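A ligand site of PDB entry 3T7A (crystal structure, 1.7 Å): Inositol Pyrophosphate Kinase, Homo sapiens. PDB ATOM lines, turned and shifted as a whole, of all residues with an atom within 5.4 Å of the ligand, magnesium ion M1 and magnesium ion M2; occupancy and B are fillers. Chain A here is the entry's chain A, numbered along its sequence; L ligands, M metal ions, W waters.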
ATOM      1  N   ARG A  98       2.033  10.647   0.139  1.00  0.00           N
ATOM      2  CA  ARG A  98       1.924  10.932  -1.298  1.00  0.00           C
ATOM      3  C   ARG A  98       2.070   9.680  -2.181  1.00  0.00           C
ATOM      4  O   ARG A  98       1.481   9.600  -3.246  1.00  0.00           O
ATOM      5  CB  ARG A  98       2.967  11.976  -1.718  1.00  0.00           C
ATOM      6  CG  ARG A  98       2.862  13.300  -0.997  1.00  0.00           C
ATOM      7  CD  ARG A  98       3.754  14.369  -1.635  1.00  0.00           C
ATOM      8  NE  ARG A  98       3.915  15.512  -0.749  1.00  0.00           N
ATOM      9  CZ  ARG A  98       3.110  16.574  -0.720  1.00  0.00           C
ATOM     10  NH1 ARG A  98       2.095  16.662  -1.572  1.00  0.00           N
ATOM     11  NH2 ARG A  98       3.324  17.564   0.146  1.00  0.00           N
ATOM     12  N   TYR A 102      -0.750   8.668  -4.987  1.00  0.00           N
ATOM     13  CA  TYR A 102      -0.437   8.478  -6.393  1.00  0.00           C
ATOM     14  C   TYR A 102      -0.783   7.054  -6.864  1.00  0.00           C
ATOM     15  O   TYR A 102      -1.269   6.865  -7.988  1.00  0.00           O
ATOM     16  CB  TYR A 102       1.032   8.839  -6.653  1.00  0.00           C
ATOM     17  CG  TYR A 102       1.229  10.293  -7.038  1.00  0.00           C
ATOM     18  CD1 TYR A 102       0.301  11.284  -6.683  1.00  0.00           C
ATOM     19  CD2 TYR A 102       2.345  10.680  -7.765  1.00  0.00           C
ATOM     20  CE1 TYR A 102       0.484  12.620  -7.082  1.00  0.00           C
ATOM     21  CE2 TYR A 102       2.537  11.993  -8.168  1.00  0.00           C
ATOM     22  CZ  TYR A 102       1.617  12.967  -7.825  1.00  0.00           C
ATOM     23  OH  TYR A 102       1.831  14.270  -8.224  1.00  0.00           O
ATOM     24  N   PRO A 113       1.264  13.358 -13.188  1.00  0.00           N
ATOM     25  CA  PRO A 113       2.623  13.500 -13.754  1.00  0.00           C
ATOM     26  C   PRO A 113       3.375  12.182 -13.713  1.00  0.00           C
ATOM     27  O   PRO A 113       3.184  11.386 -12.792  1.00  0.00           O
ATOM     28  CB  PRO A 113       3.291  14.491 -12.797  1.00  0.00           C
ATOM     29  CG  PRO A 113       2.141  15.310 -12.252  1.00  0.00           C
ATOM     30  CD  PRO A 113       1.036  14.302 -12.075  1.00  0.00           C
ATOM     31  N   VAL A 149      10.185  18.083 -10.283  1.00  0.00           N
ATOM     32  CA  VAL A 149       9.604  18.427  -8.987  1.00  0.00           C
ATOM     33  C   VAL A 149       9.974  17.337  -7.984  1.00  0.00           C
ATOM     34  O   VAL A 149       9.981  16.145  -8.313  1.00  0.00           O
ATOM     35  CB  VAL A 149       8.057  18.581  -9.092  1.00  0.00           C
ATOM     36  CG1 VAL A 149       7.457  19.080  -7.791  1.00  0.00           C
ATOM     37  CG2 VAL A 149       7.701  19.562 -10.214  1.00  0.00           C
ATOM     38  N   LYS A 151       9.003  16.074  -4.116  1.00  0.00           N
ATOM     39  CA  LYS A 151       8.027  16.190  -3.038  1.00  0.00           C
ATOM     40  C   LYS A 151       8.338  15.235  -1.907  1.00  0.00           C
ATOM     41  O   LYS A 151       8.572  14.049  -2.140  1.00  0.00           O
ATOM     42  CB  LYS A 151       6.615  15.908  -3.556  1.00  0.00           C
ATOM     43  CG  LYS A 151       6.189  16.754  -4.719  1.00  0.00           C
ATOM     44  CD  LYS A 151       4.765  16.416  -5.163  1.00  0.00           C
ATOM     45  CE  LYS A 151       4.367  17.252  -6.336  1.00  0.00           C
ATOM     46  NZ  LYS A 151       2.954  16.986  -6.736  1.00  0.00           N
ATOM     47  N   ALA A 155       2.629  13.826   2.910  1.00  0.00           N
ATOM     48  CA  ALA A 155       1.733  14.806   2.325  1.00  0.00           C
ATOM     49  C   ALA A 155       1.473  16.004   3.247  1.00  0.00           C
ATOM     50  O   ALA A 155       0.947  17.014   2.806  1.00  0.00           O
ATOM     51  CB  ALA A 155       0.414  14.141   1.912  1.00  0.00           C
ATOM     52  N   ASP A 157       3.998  17.530   4.640  1.00  0.00           N
ATOM     53  CA  ASP A 157       5.234  18.317   4.475  1.00  0.00           C
ATOM     54  C   ASP A 157       5.132  19.048   3.141  1.00  0.00           C
ATOM     55  O   ASP A 157       5.161  18.427   2.078  1.00  0.00           O
ATOM     56  CB  ASP A 157       6.455  17.375   4.534  1.00  0.00           C
ATOM     57  CG  ASP A 157       7.806  18.111   4.442  1.00  0.00           C
ATOM     58  OD1 ASP A 157       7.857  19.272   3.994  1.00  0.00           O
ATOM     59  OD2 ASP A 157       8.844  17.498   4.802  1.00  0.00           O
ATOM     60  N   HIS A 158       5.012  20.386   3.207  1.00  0.00           N
ATOM     61  CA  HIS A 158       4.751  21.204   2.031  1.00  0.00           C
ATOM     62  C   HIS A 158       5.998  21.809   1.391  1.00  0.00           C
ATOM     63  O   HIS A 158       5.917  22.678   0.524  1.00  0.00           O
ATOM     64  CB  HIS A 158       3.696  22.260   2.370  1.00  0.00           C
ATOM     65  CG  HIS A 158       2.441  21.649   2.887  1.00  0.00           C
ATOM     66  ND1 HIS A 158       1.626  20.863   2.101  1.00  0.00           N
ATOM     67  CD2 HIS A 158       1.908  21.600   4.131  1.00  0.00           C
ATOM     68  CE1 HIS A 158       0.629  20.399   2.825  1.00  0.00           C
ATOM     69  NE2 HIS A 158       0.769  20.832   4.060  1.00  0.00           N
ATOM     70  N   VAL A 160       8.047  21.455  -1.055  1.00  0.00           N
ATOM     71  CA  VAL A 160       8.151  20.903  -2.406  1.00  0.00           C
ATOM     72  C   VAL A 160       9.166  21.750  -3.162  1.00  0.00           C
ATOM     73  O   VAL A 160       9.089  22.970  -3.105  1.00  0.00           O
ATOM     74  CB  VAL A 160       6.771  20.974  -3.107  1.00  0.00           C
ATOM     75  CG1 VAL A 160       6.869  20.671  -4.572  1.00  0.00           C
ATOM     76  CG2 VAL A 160       5.766  20.026  -2.415  1.00  0.00           C
ATOM     77  N   ILE A 162      11.329  22.666  -6.815  1.00  0.00           N
ATOM     78  CA  ILE A 162      11.377  22.575  -8.259  1.00  0.00           C
ATOM     79  C   ILE A 162      12.819  22.875  -8.674  1.00  0.00           C
ATOM     80  O   ILE A 162      13.417  23.826  -8.186  1.00  0.00           O
ATOM     81  CB  ILE A 162      10.372  23.531  -8.905  1.00  0.00           C
ATOM     82  CG1 ILE A 162       8.950  23.168  -8.378  1.00  0.00           C
ATOM     83  CG2 ILE A 162      10.436  23.437 -10.436  1.00  0.00           C
ATOM     84  CD1 ILE A 162       7.828  23.883  -9.033  1.00  0.00           C
ATOM     85  N   LEU A 175       9.226  25.718  -2.328  1.00  0.00           N
ATOM     86  CA  LEU A 175       7.854  26.061  -1.929  1.00  0.00           C
ATOM     87  C   LEU A 175       7.650  25.706  -0.465  1.00  0.00           C
ATOM     88  O   LEU A 175       8.383  24.881   0.093  1.00  0.00           O
ATOM     89  CB  LEU A 175       6.842  25.285  -2.782  1.00  0.00           C
ATOM     90  CG  LEU A 175       6.640  25.648  -4.242  1.00  0.00           C
ATOM     91  CD1 LEU A 175       7.919  25.573  -5.091  1.00  0.00           C
ATOM     92  CD2 LEU A 175       5.601  24.703  -4.830  1.00  0.00           C
ATOM     93  N   GLU A 201       8.957  13.990  -9.897  1.00  0.00           N
ATOM     94  CA  GLU A 201       8.012  13.979 -10.997  1.00  0.00           C
ATOM     95  C   GLU A 201       8.303  14.997 -12.074  1.00  0.00           C
ATOM     96  O   GLU A 201       8.951  16.011 -11.838  1.00  0.00           O
ATOM     97  CB  GLU A 201       6.569  14.106 -10.514  1.00  0.00           C
ATOM     98  CG  GLU A 201       6.242  15.359  -9.800  1.00  0.00           C
ATOM     99  CD  GLU A 201       4.861  15.301  -9.142  1.00  0.00           C
ATOM    100  OE1 GLU A 201       4.014  16.115  -9.505  1.00  0.00           O
ATOM    101  OE2 GLU A 201       4.636  14.460  -8.246  1.00  0.00           O
ATOM    102  N   GLU A 202       7.780  14.692 -13.255  1.00  0.00           N
ATOM    103  CA  GLU A 202       7.892  15.612 -14.374  1.00  0.00           C
ATOM    104  C   GLU A 202       7.177  16.919 -14.081  1.00  0.00           C
ATOM    105  O   GLU A 202       6.084  16.933 -13.495  1.00  0.00           O
ATOM    106  CB  GLU A 202       7.365  14.988 -15.673  1.00  0.00           C
ATOM    107  CG  GLU A 202       5.909  14.560 -15.611  1.00  0.00           C
ATOM    108  CD  GLU A 202       5.286  14.290 -16.984  1.00  0.00           C
ATOM    109  OE1 GLU A 202       5.751  14.873 -17.989  1.00  0.00           O
ATOM    110  OE2 GLU A 202       4.304  13.519 -17.040  1.00  0.00           O
ATOM    111  N   PHE A 203       7.813  18.019 -14.467  1.00  0.00           N
ATOM    112  CA  PHE A 203       7.215  19.333 -14.338  1.00  0.00           C
ATOM    113  C   PHE A 203       6.207  19.554 -15.462  1.00  0.00           C
ATOM    114  O   PHE A 203       6.543  19.433 -16.660  1.00  0.00           O
ATOM    115  CB  PHE A 203       8.296  20.417 -14.345  1.00  0.00           C
ATOM    116  CG  PHE A 203       7.757  21.807 -14.210  1.00  0.00           C
ATOM    117  CD1 PHE A 203       7.426  22.551 -15.342  1.00  0.00           C
ATOM    118  CD2 PHE A 203       7.533  22.351 -12.959  1.00  0.00           C
ATOM    119  CE1 PHE A 203       6.901  23.825 -15.223  1.00  0.00           C
ATOM    120  CE2 PHE A 203       7.009  23.631 -12.824  1.00  0.00           C
ATOM    121  CZ  PHE A 203       6.700  24.371 -13.960  1.00  0.00           C
ATOM    122  N   MET A 204       4.973  19.850 -15.074  1.00  0.00           N
ATOM    123  CA  MET A 204       3.876  20.101 -16.014  1.00  0.00           C
ATOM    124  C   MET A 204       3.718  21.592 -16.228  1.00  0.00           C
ATOM    125  O   MET A 204       3.411  22.318 -15.280  1.00  0.00           O
ATOM    126  CB  MET A 204       2.556  19.509 -15.489  1.00  0.00           C
ATOM    127  CG  MET A 204       2.637  18.078 -14.967  1.00  0.00           C
ATOM    128  SD  MET A 204       3.358  16.883 -16.118  1.00  0.00           S
ATOM    129  CE  MET A 204       2.195  16.895 -17.476  1.00  0.00           C
ATOM    130  N   PRO A 205       3.921  22.061 -17.464  1.00  0.00           N
ATOM    131  CA  PRO A 205       3.849  23.481 -17.745  1.00  0.00           C
ATOM    132  C   PRO A 205       2.388  23.928 -17.817  1.00  0.00           C
ATOM    133  O   PRO A 205       1.624  23.401 -18.612  1.00  0.00           O
ATOM    134  CB  PRO A 205       4.532  23.606 -19.112  1.00  0.00           C
ATOM    135  CG  PRO A 205       4.261  22.313 -19.783  1.00  0.00           C
ATOM    136  CD  PRO A 205       4.201  21.269 -18.678  1.00  0.00           C
ATOM    137  N   ASP A 210      -2.641  27.200 -10.750  1.00  0.00           N
ATOM    138  CA  ASP A 210      -3.086  25.867 -10.331  1.00  0.00           C
ATOM    139  C   ASP A 210      -4.596  25.925 -10.204  1.00  0.00           C
ATOM    140  O   ASP A 210      -5.132  26.919  -9.726  1.00  0.00           O
ATOM    141  CB  ASP A 210      -2.571  25.532  -8.937  1.00  0.00           C
ATOM    142  CG  ASP A 210      -1.076  25.599  -8.827  1.00  0.00           C
ATOM    143  OD1 ASP A 210      -0.385  25.290  -9.816  1.00  0.00           O
ATOM    144  OD2 ASP A 210      -0.598  25.956  -7.716  1.00  0.00           O
ATOM    145  N   LYS A 212      -7.754  24.522  -8.210  1.00  0.00           N
ATOM    146  CA  LYS A 212      -8.106  23.927  -6.905  1.00  0.00           C
ATOM    147  C   LYS A 212      -9.533  23.448  -7.010  1.00  0.00           C
ATOM    148  O   LYS A 212     -10.426  24.218  -7.371  1.00  0.00           O
ATOM    149  CB  LYS A 212      -8.017  24.982  -5.817  1.00  0.00           C
ATOM    150  CG  LYS A 212      -6.759  25.839  -5.893  1.00  0.00           C
ATOM    151  CD  LYS A 212      -5.558  24.976  -5.710  1.00  0.00           C
ATOM    152  CE  LYS A 212      -4.326  25.749  -5.301  1.00  0.00           C
ATOM    153  NZ  LYS A 212      -3.476  24.805  -4.511  1.00  0.00           N
ATOM    154  N   SER A 228       0.420  29.956  -9.374  1.00  0.00           N
ATOM    155  CA  SER A 228       1.279  28.862  -8.941  1.00  0.00           C
ATOM    156  C   SER A 228       2.445  29.377  -8.106  1.00  0.00           C
ATOM    157  O   SER A 228       3.105  30.328  -8.518  1.00  0.00           O
ATOM    158  CB  SER A 228       1.863  28.112 -10.139  1.00  0.00           C
ATOM    159  OG  SER A 228       2.687  27.040  -9.676  1.00  0.00           O
ATOM    160  N   PRO A 229       2.720  28.740  -6.947  1.00  0.00           N
ATOM    161  CA  PRO A 229       3.950  29.007  -6.181  1.00  0.00           C
ATOM    162  C   PRO A 229       5.218  28.530  -6.914  1.00  0.00           C
ATOM    163  O   PRO A 229       6.344  28.855  -6.492  1.00  0.00           O
ATOM    164  CB  PRO A 229       3.764  28.176  -4.902  1.00  0.00           C
ATOM    165  CG  PRO A 229       2.326  27.765  -4.879  1.00  0.00           C
ATOM    166  CD  PRO A 229       1.859  27.738  -6.295  1.00  0.00           C
ATOM    167  N   ALA A 230       5.049  27.789  -7.996  1.00  0.00           N
ATOM    168  CA  ALA A 230       6.173  27.342  -8.825  1.00  0.00           C
ATOM    169  C   ALA A 230       6.786  28.529  -9.570  1.00  0.00           C
ATOM    170  O   ALA A 230       7.912  28.434 -10.069  1.00  0.00           O
ATOM    171  CB  ALA A 230       5.721  26.286  -9.825  1.00  0.00           C
ATOM    172  N   ASP A 273      -5.793  19.124  -6.352  1.00  0.00           N
ATOM    173  CA  ASP A 273      -5.182  20.093  -7.270  1.00  0.00           C
ATOM    174  C   ASP A 273      -5.123  19.523  -8.674  1.00  0.00           C
ATOM    175  O   ASP A 273      -4.822  18.339  -8.841  1.00  0.00           O
ATOM    176  CB  ASP A 273      -3.743  20.420  -6.835  1.00  0.00           C
ATOM    177  CG  ASP A 273      -3.664  21.160  -5.505  1.00  0.00           C
ATOM    178  OD1 ASP A 273      -4.596  21.918  -5.167  1.00  0.00           O
ATOM    179  OD2 ASP A 273      -2.648  21.007  -4.827  1.00  0.00           O
ATOM    180  N   LEU A 275      -3.504  20.323 -12.636  1.00  0.00           N
ATOM    181  CA  LEU A 275      -2.609  21.093 -13.475  1.00  0.00           C
ATOM    182  C   LEU A 275      -3.134  20.998 -14.880  1.00  0.00           C
ATOM    183  O   LEU A 275      -3.201  19.911 -15.443  1.00  0.00           O
ATOM    184  CB  LEU A 275      -1.196  20.526 -13.402  1.00  0.00           C
ATOM    185  CG  LEU A 275      -0.579  20.449 -11.999  1.00  0.00           C
ATOM    186  CD1 LEU A 275       0.757  19.679 -12.033  1.00  0.00           C
ATOM    187  CD2 LEU A 275      -0.446  21.852 -11.349  1.00  0.00           C
ATOM    188  N   CYS A 284      -2.264  16.444  -9.148  1.00  0.00           N
ATOM    189  CA  CYS A 284      -0.919  16.389  -8.527  1.00  0.00           C
ATOM    190  C   CYS A 284      -0.941  16.318  -6.999  1.00  0.00           C
ATOM    191  O   CYS A 284       0.111  16.200  -6.373  1.00  0.00           O
ATOM    192  CB  CYS A 284      -0.054  17.573  -9.005  1.00  0.00           C
ATOM    193  SG  CYS A 284      -0.510  19.174  -8.317  1.00  0.00           S
ATOM    194  N   ASP A 285      -2.149  16.353  -6.398  1.00  0.00           N
ATOM    195  CA  ASP A 285      -2.268  16.457  -4.950  1.00  0.00           C
ATOM    196  C   ASP A 285      -3.721  16.165  -4.588  1.00  0.00           C
ATOM    197  O   ASP A 285      -4.637  16.712  -5.219  1.00  0.00           O
ATOM    198  CB  ASP A 285      -1.890  17.892  -4.535  1.00  0.00           C
ATOM    199  CG  ASP A 285      -1.788  18.108  -3.041  1.00  0.00           C
ATOM    200  OD1 ASP A 285      -1.570  17.153  -2.256  1.00  0.00           O
ATOM    201  OD2 ASP A 285      -1.867  19.298  -2.621  1.00  0.00           O
ATOM    202  N   VAL A 286      -3.938  15.282  -3.625  1.00  0.00           N
ATOM    203  CA  VAL A 286      -5.276  15.031  -3.071  1.00  0.00           C
ATOM    204  C   VAL A 286      -5.185  15.304  -1.575  1.00  0.00           C
ATOM    205  O   VAL A 286      -4.360  14.696  -0.878  1.00  0.00           O
ATOM    206  CB  VAL A 286      -5.769  13.571  -3.323  1.00  0.00           C
ATOM    207  CG1 VAL A 286      -7.157  13.345  -2.652  1.00  0.00           C
ATOM    208  CG2 VAL A 286      -5.827  13.248  -4.818  1.00  0.00           C
ATOM    209  N   ASN A 287      -6.012  16.223  -1.075  1.00  0.00           N
ATOM    210  CA  ASN A 287      -5.894  16.685   0.298  1.00  0.00           C
ATOM    211  C   ASN A 287      -6.976  16.224   1.249  1.00  0.00           C
ATOM    212  O   ASN A 287      -6.847  16.418   2.464  1.00  0.00           O
ATOM    213  CB  ASN A 287      -5.800  18.217   0.297  1.00  0.00           C
ATOM    214  CG  ASN A 287      -4.591  18.686  -0.449  1.00  0.00           C
ATOM    215  OD1 ASN A 287      -3.479  18.177  -0.233  1.00  0.00           O
ATOM    216  ND2 ASN A 287      -4.775  19.662  -1.343  1.00  0.00           N
HETATM  217  P1  LIG L   1       1.085  20.349  -1.448  1.00  0.00           P
HETATM  218  O1  LIG L   1       2.216  20.872  -0.495  1.00  0.00           O
HETATM  219  O2  LIG L   1       0.506  19.041  -0.772  1.00  0.00           O
HETATM  220  O3  LIG L   1       0.034  21.376  -1.746  1.00  0.00           O
HETATM  221  P2  LIG L   1       1.482  19.891  -4.295  1.00  0.00           P
HETATM  222  O4  LIG L   1       1.662  18.514  -4.797  1.00  0.00           O
HETATM  223  O5  LIG L   1       0.169  20.536  -4.485  1.00  0.00           O
HETATM  224  O6  LIG L   1       1.932  19.876  -2.761  1.00  0.00           O
HETATM  225  O7  LIG L   1       2.636  20.826  -4.880  1.00  0.00           O
HETATM  226  C1  LIG L   1       2.622  22.265  -4.597  1.00  0.00           C
HETATM  227  C2  LIG L   1       2.563  23.135  -5.870  1.00  0.00           C
HETATM  228  O8  LIG L   1       3.711  22.785  -6.664  1.00  0.00           O
HETATM  229  C3  LIG L   1       1.374  22.790  -6.750  1.00  0.00           C
HETATM  230  O9  LIG L   1       0.215  23.516  -6.335  1.00  0.00           O
HETATM  231  C4  LIG L   1       1.881  23.261  -8.103  1.00  0.00           C
HETATM  232  O10 LIG L   1       1.885  24.690  -8.197  1.00  0.00           O
HETATM  233  C5  LIG L   1       3.342  22.796  -8.055  1.00  0.00           C
HETATM  234  N1  LIG L   1       3.424  21.436  -8.629  1.00  0.00           N
HETATM  235  C6  LIG L   1       3.229  20.173  -7.898  1.00  0.00           C
HETATM  236  N2  LIG L   1       3.655  19.177  -8.864  1.00  0.00           N
HETATM  237  C7  LIG L   1       3.887  19.780 -10.032  1.00  0.00           C
HETATM  238  C8  LIG L   1       4.236  19.281 -11.269  1.00  0.00           C
HETATM  239  N3  LIG L   1       4.410  17.977 -11.450  1.00  0.00           N
HETATM  240  N4  LIG L   1       4.400  20.152 -12.281  1.00  0.00           N
HETATM  241  C9  LIG L   1       4.230  21.468 -12.129  1.00  0.00           C
HETATM  242  N5  LIG L   1       3.919  21.996 -10.937  1.00  0.00           N
HETATM  243  C10 LIG L   1       3.732  21.165  -9.896  1.00  0.00           C
HETATM  244 MG    MG M   1      -1.434  18.623  -0.398  1.00  0.00          MG
HETATM  245 MG    MG M   2      -1.383  21.208  -3.285  1.00  0.00          MG
HETATM  246  O   HOH W   1      -1.031  23.210  -4.006  1.00  0.00           O
HETATM  247  O   HOH W   2       0.175  23.681   0.093  1.00  0.00           O
HETATM  248  O   HOH W   3       2.737  25.120  -2.607  1.00  0.00           O
HETATM  249  O   HOH W   4      -1.001  17.202   0.852  1.00  0.00           O
HETATM  250  O   HOH W   5       3.836  22.887  -1.377  1.00  0.00           O
HETATM  251  O   HOH W   6      -1.836  20.162   0.601  1.00  0.00           O
HETATM  252  O   HOH W   7       1.171  15.222  -4.034  1.00  0.00           O
HETATM  253  O   HOH W   8      -1.015  26.218  -5.312  1.00  0.00           O
HETATM  254  O   HOH W   9      -2.804  21.974  -1.934  1.00  0.00           O
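ND1 of His 158 sits at hydrogen-bond distance from O1 of the ligand (2.7 Å).
A nitrogen (N3) of the ligand sits at hydrogen-bond distance from the side-chain carboxylate of Glu 201 (2.7 Å).
NZ of Lys 151 is in salt-bridge range of O4 of the ligand (2.8 Å).
OD2 of Asp 210 sits at hydrogen-bond distance from O10 of the ligand (2.8 Å).
O of Glu 202 lies within hydrogen-bond range of N3 of the ligand (2.8 Å).
N of Met 204 lies within hydrogen-bond range of N4 of the ligand, at 2.9 Å.
An oxygen (O10) of the ligand lies within hydrogen-bond range of the side-chain hydroxyl (OG) of Ser 228 (2.9 Å).
O1 of the ligand lies within salt-bridge range of NH2 of Arg 98.
NZ of Lys 212 lies within salt-bridge range of OD1 of Asp 273 (3.2 Å).
OD1 of Asp 285 lies close to NH1 of Arg 98.
The side-chain carboxylate (OE1) of Glu 201 lies within salt-bridge range of the side-chain amino group (NZ) of Lys 151 (3.1 Å).
The side-chain hydroxyl of Tyr 102 lies within hydrogen-bond range of the side-chain carboxylate of Glu 201.
The side-chain amino group (NZ) of Lys 151 sits at hydrogen-bond distance from the backbone carbonyl oxygen (O) of Cys 284.
OH of Tyr 102 lies within hydrogen-bond range of NZ of Lys 151 (3.3 Å).
N of Ala 230 is in hydrogen-bond range of OG of Ser 228, at 3.0 Å.
O of Asp 157 lies within hydrogen-bond range of NH2 of Arg 98 (2.8 Å).
The backbone carbonyl oxygen (O) of Cys 284 sits close to an oxygen (O4) of the ligand (3.2 Å).
Residues that only touch the ligand: Leu 175, Phe 203, Leu 275, Pro 113, Pro 229, Val 149 and Val 160.
Hydrophobic or aromatic side chains within 4 Å of the ligand: Pro 113, Val 149, His 158, Val 160, Leu 175, Phe 203, Met 204, Pro 229 and Leu 275.
Two residues have an atom within 4 Å of magnesium ion M1: Asp 285 and Asn 287.
The nearest printed residue that does not touch magnesium ion M1 is Arg 98 (4.2 Å).
Of the 27 residues printed, 2 come within 4 Å of magnesium ion M2.
The nearest printed residue that does not touch magnesium ion M2 is Asn 287 (4.2 Å).
Water W6 is bound to magnesium ion M1 (1.9 Å).
Water W4 binds magnesium ion M1 (1.9 Å).
O2 of the ligand is bound to magnesium ion M1.
Magnesium ion M1 is bound by OD1 of Asn 287.
Magnesium ion M1 is bound by the side-chain carboxylate (OD2) of Asp 285 (2.4 Å).
OD1 of Asp 285 binds magnesium ion M1.
Magnesium ion M2 is bound by OD2 of Asp 273 (2.0 Å), O5 of the ligand (2.1 Å), OD2 of Asp 285 (2.1 Å), O3 of the ligand (2.1 Å), water W9 (2.1 Å) and water W1 (2.2 Å).
Magnesium ion M2 has six donor atoms within binding distance.
Water W1 bridges O9 of the ligand (2.7 Å) and NZ of Lys 212 (3.0 Å).
Water W5 bridges O1 of the ligand (2.7 Å) and O of His 158 (2.8 Å).
Water W8 lies within hydrogen-bond range of the side-chain carboxylate (OD2) of Asp 210 (2.5 Å), the side-chain amino group (NZ) of Lys 212 (2.9 Å) and an oxygen (O9) of the ligand (3.1 Å).
Water W7 lies within hydrogen-bond range of the backbone carbonyl oxygen of Cys 284, the guanidinium group of Arg 98 and an oxygen (O4) of the ligand.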
